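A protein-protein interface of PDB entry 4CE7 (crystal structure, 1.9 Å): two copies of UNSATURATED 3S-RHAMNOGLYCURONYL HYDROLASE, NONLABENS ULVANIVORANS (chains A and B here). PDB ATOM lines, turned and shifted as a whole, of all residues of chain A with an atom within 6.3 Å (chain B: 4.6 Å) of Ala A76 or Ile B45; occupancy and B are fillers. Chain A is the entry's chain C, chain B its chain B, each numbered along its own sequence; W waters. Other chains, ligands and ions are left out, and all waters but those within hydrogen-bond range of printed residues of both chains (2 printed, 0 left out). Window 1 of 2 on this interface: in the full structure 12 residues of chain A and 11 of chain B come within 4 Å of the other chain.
The backbone carbonyl oxygen (O) of Phe B46 lies within hydrogen-bond range of the side-chain amino group (NZ) of Lys A79, 3.1 Å away. SD of Met A72 sits close to O of Tyr B351 (3.8 Å).
The backbone carbonyl oxygen (O) of His B43 is in hydrogen-bond range of the side-chain amide nitrogen (NE2) of Gln B40. The backbone carbonyl oxygen (O) of Gln B352 sits close to the side-chain amide oxygen (OE1) of Gln B40, at 3.4 Å. The backbone carbonyl oxygen (O) of Ile B45 is in hydrogen-bond range of the side-chain amide nitrogen (ND2) of Asn B55, 2.9 Å away. The backbone carbonyl oxygen of Ile B45 is in hydrogen-bond range of the side-chain amide nitrogen of Asn B353. The side-chain amide nitrogen of Gln B352 lies within hydrogen-bond range of the side-chain amide oxygen of Asn B353. The side-chain amide oxygen (OD1) of Asn A71 is in hydrogen-bond range of the backbone NH (N) of Met A73 (2.8 Å).
Among the printed residues, merely in contact across the chains: Met A72 with Ile B45, Met A72 with Gln B352, Met A73 with His B43, Met A73 with Tyr B351, Ala A76 with Pro B44, Ala A76 with Ile B45, Asn A80 with Pro B44 and Asn A80 with Phe B46.
Of the printed residues of chain B, Met A72 touches Ile B45, Tyr B351 and Gln B352. Printed residues of chain B within 4 Å of Met A73: His B43 and Tyr B351. Of the printed residues of chain B, Ala A76 touches Pro B44 (3.97 Å) and Ile B45 (3.7 Å). Ala A77 touches none of the printed residues of chain B. Of the printed residues of chain B, Lys A79 touches Phe B46 (3.1 Å). Gln B40 touches none of the printed residues of chain A. Printed residues of chain A within 4 Å of Phe B46: Lys A79 and Asn A80. The nearest residue of chain B that does not touch Ala A76 is Tyr B351 (4.4 Å).
Hydrophobic or aromatic side chains of chain B that line the printed part of chain A: His B43, Pro B44, Ile B45, Phe B46 and Tyr B351. Along chain B the printed residues that touch a printed residue of chain A span positions 43 to 352. Hydrophobic or aromatic side chains of chain A that line the printed part of chain B: Met A72, Met A73 and Ala A76. Along chain A the printed residues that touch a printed residue of chain B span positions 72 to 80.
No position is printed for both chains. Of the 10 pairs that touch across the chains among the printed residues, none has its exchanged pair printed and touching as well.
Water W2 lies within hydrogen-bond range of NZ of Lys A79 and O of Phe B46. Water W1 bridges N of Phe B46 and O of Ala A76.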
ATOM      1  N   ASN A  71     -19.349  24.670  32.377  1.00  0.00           N
ATOM      2  CA  ASN A  71     -20.754  24.427  32.098  1.00  0.00           C
ATOM      3  C   ASN A  71     -20.911  22.911  31.869  1.00  0.00           C
ATOM      4  O   ASN A  71     -20.217  22.336  31.052  1.00  0.00           O
ATOM      5  CB  ASN A  71     -21.180  25.179  30.844  1.00  0.00           C
ATOM      6  CG  ASN A  71     -22.672  25.096  30.584  1.00  0.00           C
ATOM      7  OD1 ASN A  71     -23.316  24.032  30.701  1.00  0.00           O
ATOM      8  ND2 ASN A  71     -23.243  26.224  30.231  1.00  0.00           N
ATOM      9  N   MET A  72     -21.836  22.303  32.628  1.00  0.00           N
ATOM     10  CA  MET A  72     -22.078  20.873  32.668  1.00  0.00           C
ATOM     11  C   MET A  72     -22.456  20.382  31.270  1.00  0.00           C
ATOM     12  O   MET A  72     -22.234  19.211  30.965  1.00  0.00           O
ATOM     13  CB  MET A  72     -23.203  20.517  33.693  1.00  0.00           C
ATOM     14  CG  MET A  72     -24.591  21.005  33.259  1.00  0.00           C
ATOM     15  SD  MET A  72     -25.855  20.641  34.501  1.00  0.00           S
ATOM     16  CE  MET A  72     -26.213  18.981  34.030  1.00  0.00           C
ATOM     17  N   MET A  73     -23.019  21.245  30.420  1.00  0.00           N
ATOM     18  CA  MET A  73     -23.338  20.850  29.073  1.00  0.00           C
ATOM     19  C   MET A  73     -22.114  20.358  28.242  1.00  0.00           C
ATOM     20  O   MET A  73     -22.232  19.411  27.421  1.00  0.00           O
ATOM     21  CB  MET A  73     -24.028  21.981  28.325  1.00  0.00           C
ATOM     22  CG  MET A  73     -24.695  21.519  27.044  1.00  0.00           C
ATOM     23  SD  MET A  73     -25.611  22.737  26.050  1.00  0.00           S
ATOM     24  CE  MET A  73     -26.810  23.365  27.263  1.00  0.00           C
ATOM     25  N   TYR A  74     -20.980  21.040  28.387  1.00  0.00           N
ATOM     26  CA  TYR A  74     -19.784  20.682  27.661  1.00  0.00           C
ATOM     27  C   TYR A  74     -19.323  19.300  28.143  1.00  0.00           C
ATOM     28  O   TYR A  74     -18.953  18.454  27.317  1.00  0.00           O
ATOM     29  CB  TYR A  74     -18.649  21.686  27.907  1.00  0.00           C
ATOM     30  CG  TYR A  74     -18.904  23.017  27.273  1.00  0.00           C
ATOM     31  CD1 TYR A  74     -19.054  23.151  25.849  1.00  0.00           C
ATOM     32  CD2 TYR A  74     -19.095  24.145  28.084  1.00  0.00           C
ATOM     33  CE1 TYR A  74     -19.301  24.395  25.275  1.00  0.00           C
ATOM     34  CE2 TYR A  74     -19.332  25.370  27.518  1.00  0.00           C
ATOM     35  CZ  TYR A  74     -19.450  25.499  26.138  1.00  0.00           C
ATOM     36  OH  TYR A  74     -19.716  26.749  25.631  1.00  0.00           O
ATOM     37  N   MET A  75     -19.318  19.088  29.472  1.00  0.00           N
ATOM     38  CA  MET A  75     -18.859  17.820  30.089  1.00  0.00           C
ATOM     39  C   MET A  75     -19.778  16.634  29.725  1.00  0.00           C
ATOM     40  O   MET A  75     -19.300  15.533  29.531  1.00  0.00           O
ATOM     41  CB  MET A  75     -18.745  17.981  31.635  1.00  0.00           C
ATOM     42  CG  MET A  75     -18.274  16.707  32.343  1.00  0.00           C
ATOM     43  SD  MET A  75     -16.651  16.090  31.673  1.00  0.00           S
ATOM     44  CE  MET A  75     -15.513  17.219  32.558  1.00  0.00           C
ATOM     45  N   ALA A  76     -21.092  16.879  29.591  1.00  0.00           N
ATOM     46  CA  ALA A  76     -22.060  15.842  29.183  1.00  0.00           C
ATOM     47  C   ALA A  76     -21.675  15.395  27.761  1.00  0.00           C
ATOM     48  O   ALA A  76     -21.594  14.200  27.467  1.00  0.00           O
ATOM     49  CB  ALA A  76     -23.501  16.393  29.214  1.00  0.00           C
ATOM     50  N   ALA A  77     -21.391  16.357  26.890  1.00  0.00           N
ATOM     51  CA  ALA A  77     -21.035  16.021  25.509  1.00  0.00           C
ATOM     52  C   ALA A  77     -19.702  15.206  25.445  1.00  0.00           C
ATOM     53  O   ALA A  77     -19.574  14.217  24.641  1.00  0.00           O
ATOM     54  CB  ALA A  77     -20.920  17.319  24.691  1.00  0.00           C
ATOM     55  N   LEU A  78     -18.743  15.601  26.289  1.00  0.00           N
ATOM     56  CA  LEU A  78     -17.400  14.959  26.359  1.00  0.00           C
ATOM     57  C   LEU A  78     -17.596  13.514  26.877  1.00  0.00           C
ATOM     58  O   LEU A  78     -17.108  12.573  26.278  1.00  0.00           O
ATOM     59  CB  LEU A  78     -16.453  15.781  27.306  1.00  0.00           C
ATOM     60  CG  LEU A  78     -15.897  17.077  26.685  1.00  0.00           C
ATOM     61  CD1 LEU A  78     -15.276  17.957  27.778  1.00  0.00           C
ATOM     62  CD2 LEU A  78     -14.830  16.851  25.595  1.00  0.00           C
ATOM     63  N   LYS A  79     -18.364  13.355  27.970  1.00  0.00           N
ATOM     64  CA  LYS A  79     -18.597  12.032  28.544  1.00  0.00           C
ATOM     65  C   LYS A  79     -19.363  11.195  27.497  1.00  0.00           C
ATOM     66  O   LYS A  79     -19.058  10.011  27.298  1.00  0.00           O
ATOM     67  CB  LYS A  79     -19.375  12.090  29.884  1.00  0.00           C
ATOM     68  CG  LYS A  79     -18.489  12.659  30.983  1.00  0.00           C
ATOM     69  CD  LYS A  79     -19.335  13.098  32.196  1.00  0.00           C
ATOM     70  CE  LYS A  79     -20.077  11.895  32.773  1.00  0.00           C
ATOM     71  NZ  LYS A  79     -20.831  12.291  33.970  1.00  0.00           N
ATOM     72  N   ASN A  80     -20.417  11.753  26.894  1.00  0.00           N
ATOM     73  CA  ASN A  80     -21.225  11.009  25.896  1.00  0.00           C
ATOM     74  C   ASN A  80     -20.345  10.327  24.828  1.00  0.00           C
ATOM     75  O   ASN A  80     -20.475   9.109  24.524  1.00  0.00           O
ATOM     76  CB  ASN A  80     -22.176  11.993  25.190  1.00  0.00           C
ATOM     77  CG  ASN A  80     -23.300  11.312  24.395  1.00  0.00           C
ATOM     78  OD1 ASN A  80     -23.983  10.415  24.882  1.00  0.00           O
ATOM     79  ND2 ASN A  80     -23.556  11.822  23.214  1.00  0.00           N
ATOM     80  N   GLN A  81     -19.495  11.134  24.197  1.00  0.00           N
ATOM     81  CA  GLN A  81     -18.706  10.595  23.030  1.00  0.00           C
ATOM     82  C   GLN A  81     -17.632   9.601  23.563  1.00  0.00           C
ATOM     83  O   GLN A  81     -17.337   8.592  22.953  1.00  0.00           O
ATOM     84  CB  GLN A  81     -18.086  11.695  22.185  1.00  0.00           C
ATOM     85  CG  GLN A  81     -17.092  12.658  22.873  1.00  0.00           C
ATOM     86  CD  GLN A  81     -15.634  12.171  22.945  1.00  0.00           C
ATOM     87  OE1 GLN A  81     -14.910  12.467  23.934  1.00  0.00           O
ATOM     88  NE2 GLN A  81     -15.183  11.471  21.925  1.00  0.00           N
ATOM     89  N   GLN B  40     -34.377  17.603  25.887  1.00  0.00           N
ATOM     90  CA  GLN B  40     -33.571  16.582  26.567  1.00  0.00           C
ATOM     91  C   GLN B  40     -33.014  15.516  25.596  1.00  0.00           C
ATOM     92  O   GLN B  40     -31.884  15.048  25.762  1.00  0.00           O
ATOM     93  CB  GLN B  40     -34.356  15.879  27.669  1.00  0.00           C
ATOM     94  CG  GLN B  40     -33.439  15.097  28.645  1.00  0.00           C
ATOM     95  CD  GLN B  40     -32.474  16.020  29.362  1.00  0.00           C
ATOM     96  OE1 GLN B  40     -32.888  16.731  30.279  1.00  0.00           O
ATOM     97  NE2 GLN B  40     -31.198  16.002  28.984  1.00  0.00           N
ATOM     98  N   HIS B  43     -29.913  16.804  24.257  1.00  0.00           N
ATOM     99  CA  HIS B  43     -28.848  16.981  25.273  1.00  0.00           C
ATOM    100  C   HIS B  43     -28.653  15.763  26.139  1.00  0.00           C
ATOM    101  O   HIS B  43     -28.805  15.865  27.343  1.00  0.00           O
ATOM    102  CB  HIS B  43     -29.194  18.173  26.188  1.00  0.00           C
ATOM    103  CG  HIS B  43     -29.254  19.485  25.451  1.00  0.00           C
ATOM    104  ND1 HIS B  43     -30.360  19.845  24.692  1.00  0.00           N
ATOM    105  CD2 HIS B  43     -28.351  20.567  25.382  1.00  0.00           C
ATOM    106  CE1 HIS B  43     -30.132  21.058  24.107  1.00  0.00           C
ATOM    107  NE2 HIS B  43     -28.920  21.522  24.556  1.00  0.00           N
ATOM    108  N   PRO B  44     -28.330  14.605  25.543  1.00  0.00           N
ATOM    109  CA  PRO B  44     -28.208  13.384  26.345  1.00  0.00           C
ATOM    110  C   PRO B  44     -27.154  13.524  27.412  1.00  0.00           C
ATOM    111  O   PRO B  44     -26.124  14.191  27.212  1.00  0.00           O
ATOM    112  CB  PRO B  44     -27.768  12.312  25.326  1.00  0.00           C
ATOM    113  CG  PRO B  44     -27.155  13.120  24.161  1.00  0.00           C
ATOM    114  CD  PRO B  44     -27.924  14.424  24.119  1.00  0.00           C
ATOM    115  N   ILE B  45     -27.373  12.882  28.542  1.00  0.00           N
ATOM    116  CA  ILE B  45     -26.506  13.095  29.678  1.00  0.00           C
ATOM    117  C   ILE B  45     -26.667  11.821  30.574  1.00  0.00           C
ATOM    118  O   ILE B  45     -27.676  11.118  30.484  1.00  0.00           O
ATOM    119  CB  ILE B  45     -26.867  14.396  30.454  1.00  0.00           C
ATOM    120  CG1 ILE B  45     -25.831  14.726  31.592  1.00  0.00           C
ATOM    121  CG2 ILE B  45     -28.344  14.342  30.985  1.00  0.00           C
ATOM    122  CD1 ILE B  45     -26.007  16.181  32.120  1.00  0.00           C
ATOM    123  N   PHE B  46     -25.648  11.530  31.364  1.00  0.00           N
ATOM    124  CA  PHE B  46     -25.708  10.439  32.340  1.00  0.00           C
ATOM    125  C   PHE B  46     -24.668  10.738  33.399  1.00  0.00           C
ATOM    126  O   PHE B  46     -23.732  11.526  33.158  1.00  0.00           O
ATOM    127  CB  PHE B  46     -25.365   9.102  31.657  1.00  0.00           C
ATOM    128  CG  PHE B  46     -24.122   9.124  30.781  1.00  0.00           C
ATOM    129  CD1 PHE B  46     -22.849   9.030  31.333  1.00  0.00           C
ATOM    130  CD2 PHE B  46     -24.237   9.086  29.374  1.00  0.00           C
ATOM    131  CE1 PHE B  46     -21.701   9.042  30.522  1.00  0.00           C
ATOM    132  CE2 PHE B  46     -23.084   9.048  28.568  1.00  0.00           C
ATOM    133  CZ  PHE B  46     -21.839   9.006  29.144  1.00  0.00           C
ATOM    134  N   THR B  54     -30.138   7.946  36.187  1.00  0.00           N
ATOM    135  CA  THR B  54     -30.500   9.294  35.738  1.00  0.00           C
ATOM    136  C   THR B  54     -31.350   9.109  34.476  1.00  0.00           C
ATOM    137  O   THR B  54     -32.425   9.751  34.342  1.00  0.00           O
ATOM    138  CB  THR B  54     -29.302  10.262  35.549  1.00  0.00           C
ATOM    139  OG1 THR B  54     -28.517   9.929  34.362  1.00  0.00           O
ATOM    140  CG2 THR B  54     -28.405  10.332  36.832  1.00  0.00           C
ATOM    141  N   ASN B  55     -30.941   8.177  33.604  1.00  0.00           N
ATOM    142  CA  ASN B  55     -31.743   7.950  32.384  1.00  0.00           C
ATOM    143  C   ASN B  55     -32.969   7.091  32.699  1.00  0.00           C
ATOM    144  O   ASN B  55     -33.966   7.199  32.015  1.00  0.00           O
ATOM    145  CB  ASN B  55     -30.901   7.324  31.263  1.00  0.00           C
ATOM    146  CG  ASN B  55     -29.994   8.350  30.635  1.00  0.00           C
ATOM    147  OD1 ASN B  55     -30.475   9.198  29.857  1.00  0.00           O
ATOM    148  ND2 ASN B  55     -28.769   8.476  31.190  1.00  0.00           N
ATOM    149  N   TYR B 351     -30.288  21.954  34.787  1.00  0.00           N
ATOM    150  CA  TYR B 351     -31.170  20.967  34.215  1.00  0.00           C
ATOM    151  C   TYR B 351     -30.612  19.621  34.573  1.00  0.00           C
ATOM    152  O   TYR B 351     -29.444  19.504  34.992  1.00  0.00           O
ATOM    153  CB  TYR B 351     -31.247  21.068  32.662  1.00  0.00           C
ATOM    154  CG  TYR B 351     -29.974  20.696  31.916  1.00  0.00           C
ATOM    155  CD1 TYR B 351     -28.945  21.633  31.724  1.00  0.00           C
ATOM    156  CD2 TYR B 351     -29.764  19.359  31.465  1.00  0.00           C
ATOM    157  CE1 TYR B 351     -27.774  21.297  31.020  1.00  0.00           C
ATOM    158  CE2 TYR B 351     -28.598  18.997  30.797  1.00  0.00           C
ATOM    159  CZ  TYR B 351     -27.588  19.973  30.587  1.00  0.00           C
ATOM    160  OH  TYR B 351     -26.439  19.622  29.884  1.00  0.00           O
ATOM    161  N   GLN B 352     -31.434  18.603  34.377  1.00  0.00           N
ATOM    162  CA  GLN B 352     -30.874  17.242  34.360  1.00  0.00           C
ATOM    163  C   GLN B 352     -31.913  16.380  33.697  1.00  0.00           C
ATOM    164  O   GLN B 352     -33.084  16.771  33.675  1.00  0.00           O
ATOM    165  CB  GLN B 352     -30.679  16.736  35.774  1.00  0.00           C
ATOM    166  CG  GLN B 352     -29.186  16.721  36.345  1.00  0.00           C
ATOM    167  CD  GLN B 352     -28.209  15.768  35.577  1.00  0.00           C
ATOM    168  OE1 GLN B 352     -26.957  15.732  35.908  1.00  0.00           O
ATOM    169  NE2 GLN B 352     -28.722  14.977  34.602  1.00  0.00           N
ATOM    170  N   ASN B 353     -31.498  15.212  33.193  1.00  0.00           N
ATOM    171  CA  ASN B 353     -32.426  14.333  32.495  1.00  0.00           C
ATOM    172  C   ASN B 353     -33.546  13.869  33.467  1.00  0.00           C
ATOM    173  O   ASN B 353     -34.717  13.865  33.085  1.00  0.00           O
ATOM    174  CB  ASN B 353     -31.671  13.155  31.808  1.00  0.00           C
ATOM    175  CG  ASN B 353     -30.773  12.359  32.780  1.00  0.00           C
ATOM    176  OD1 ASN B 353     -30.668  12.660  33.992  1.00  0.00           O
ATOM    177  ND2 ASN B 353     -30.099  11.332  32.236  1.00  0.00           N
HETATM  178  O   HOH W   1     -22.915  12.631  30.167  1.00  0.00           O
HETATM  179  O   HOH W   2     -22.620  14.326  32.943  1.00  0.00           O
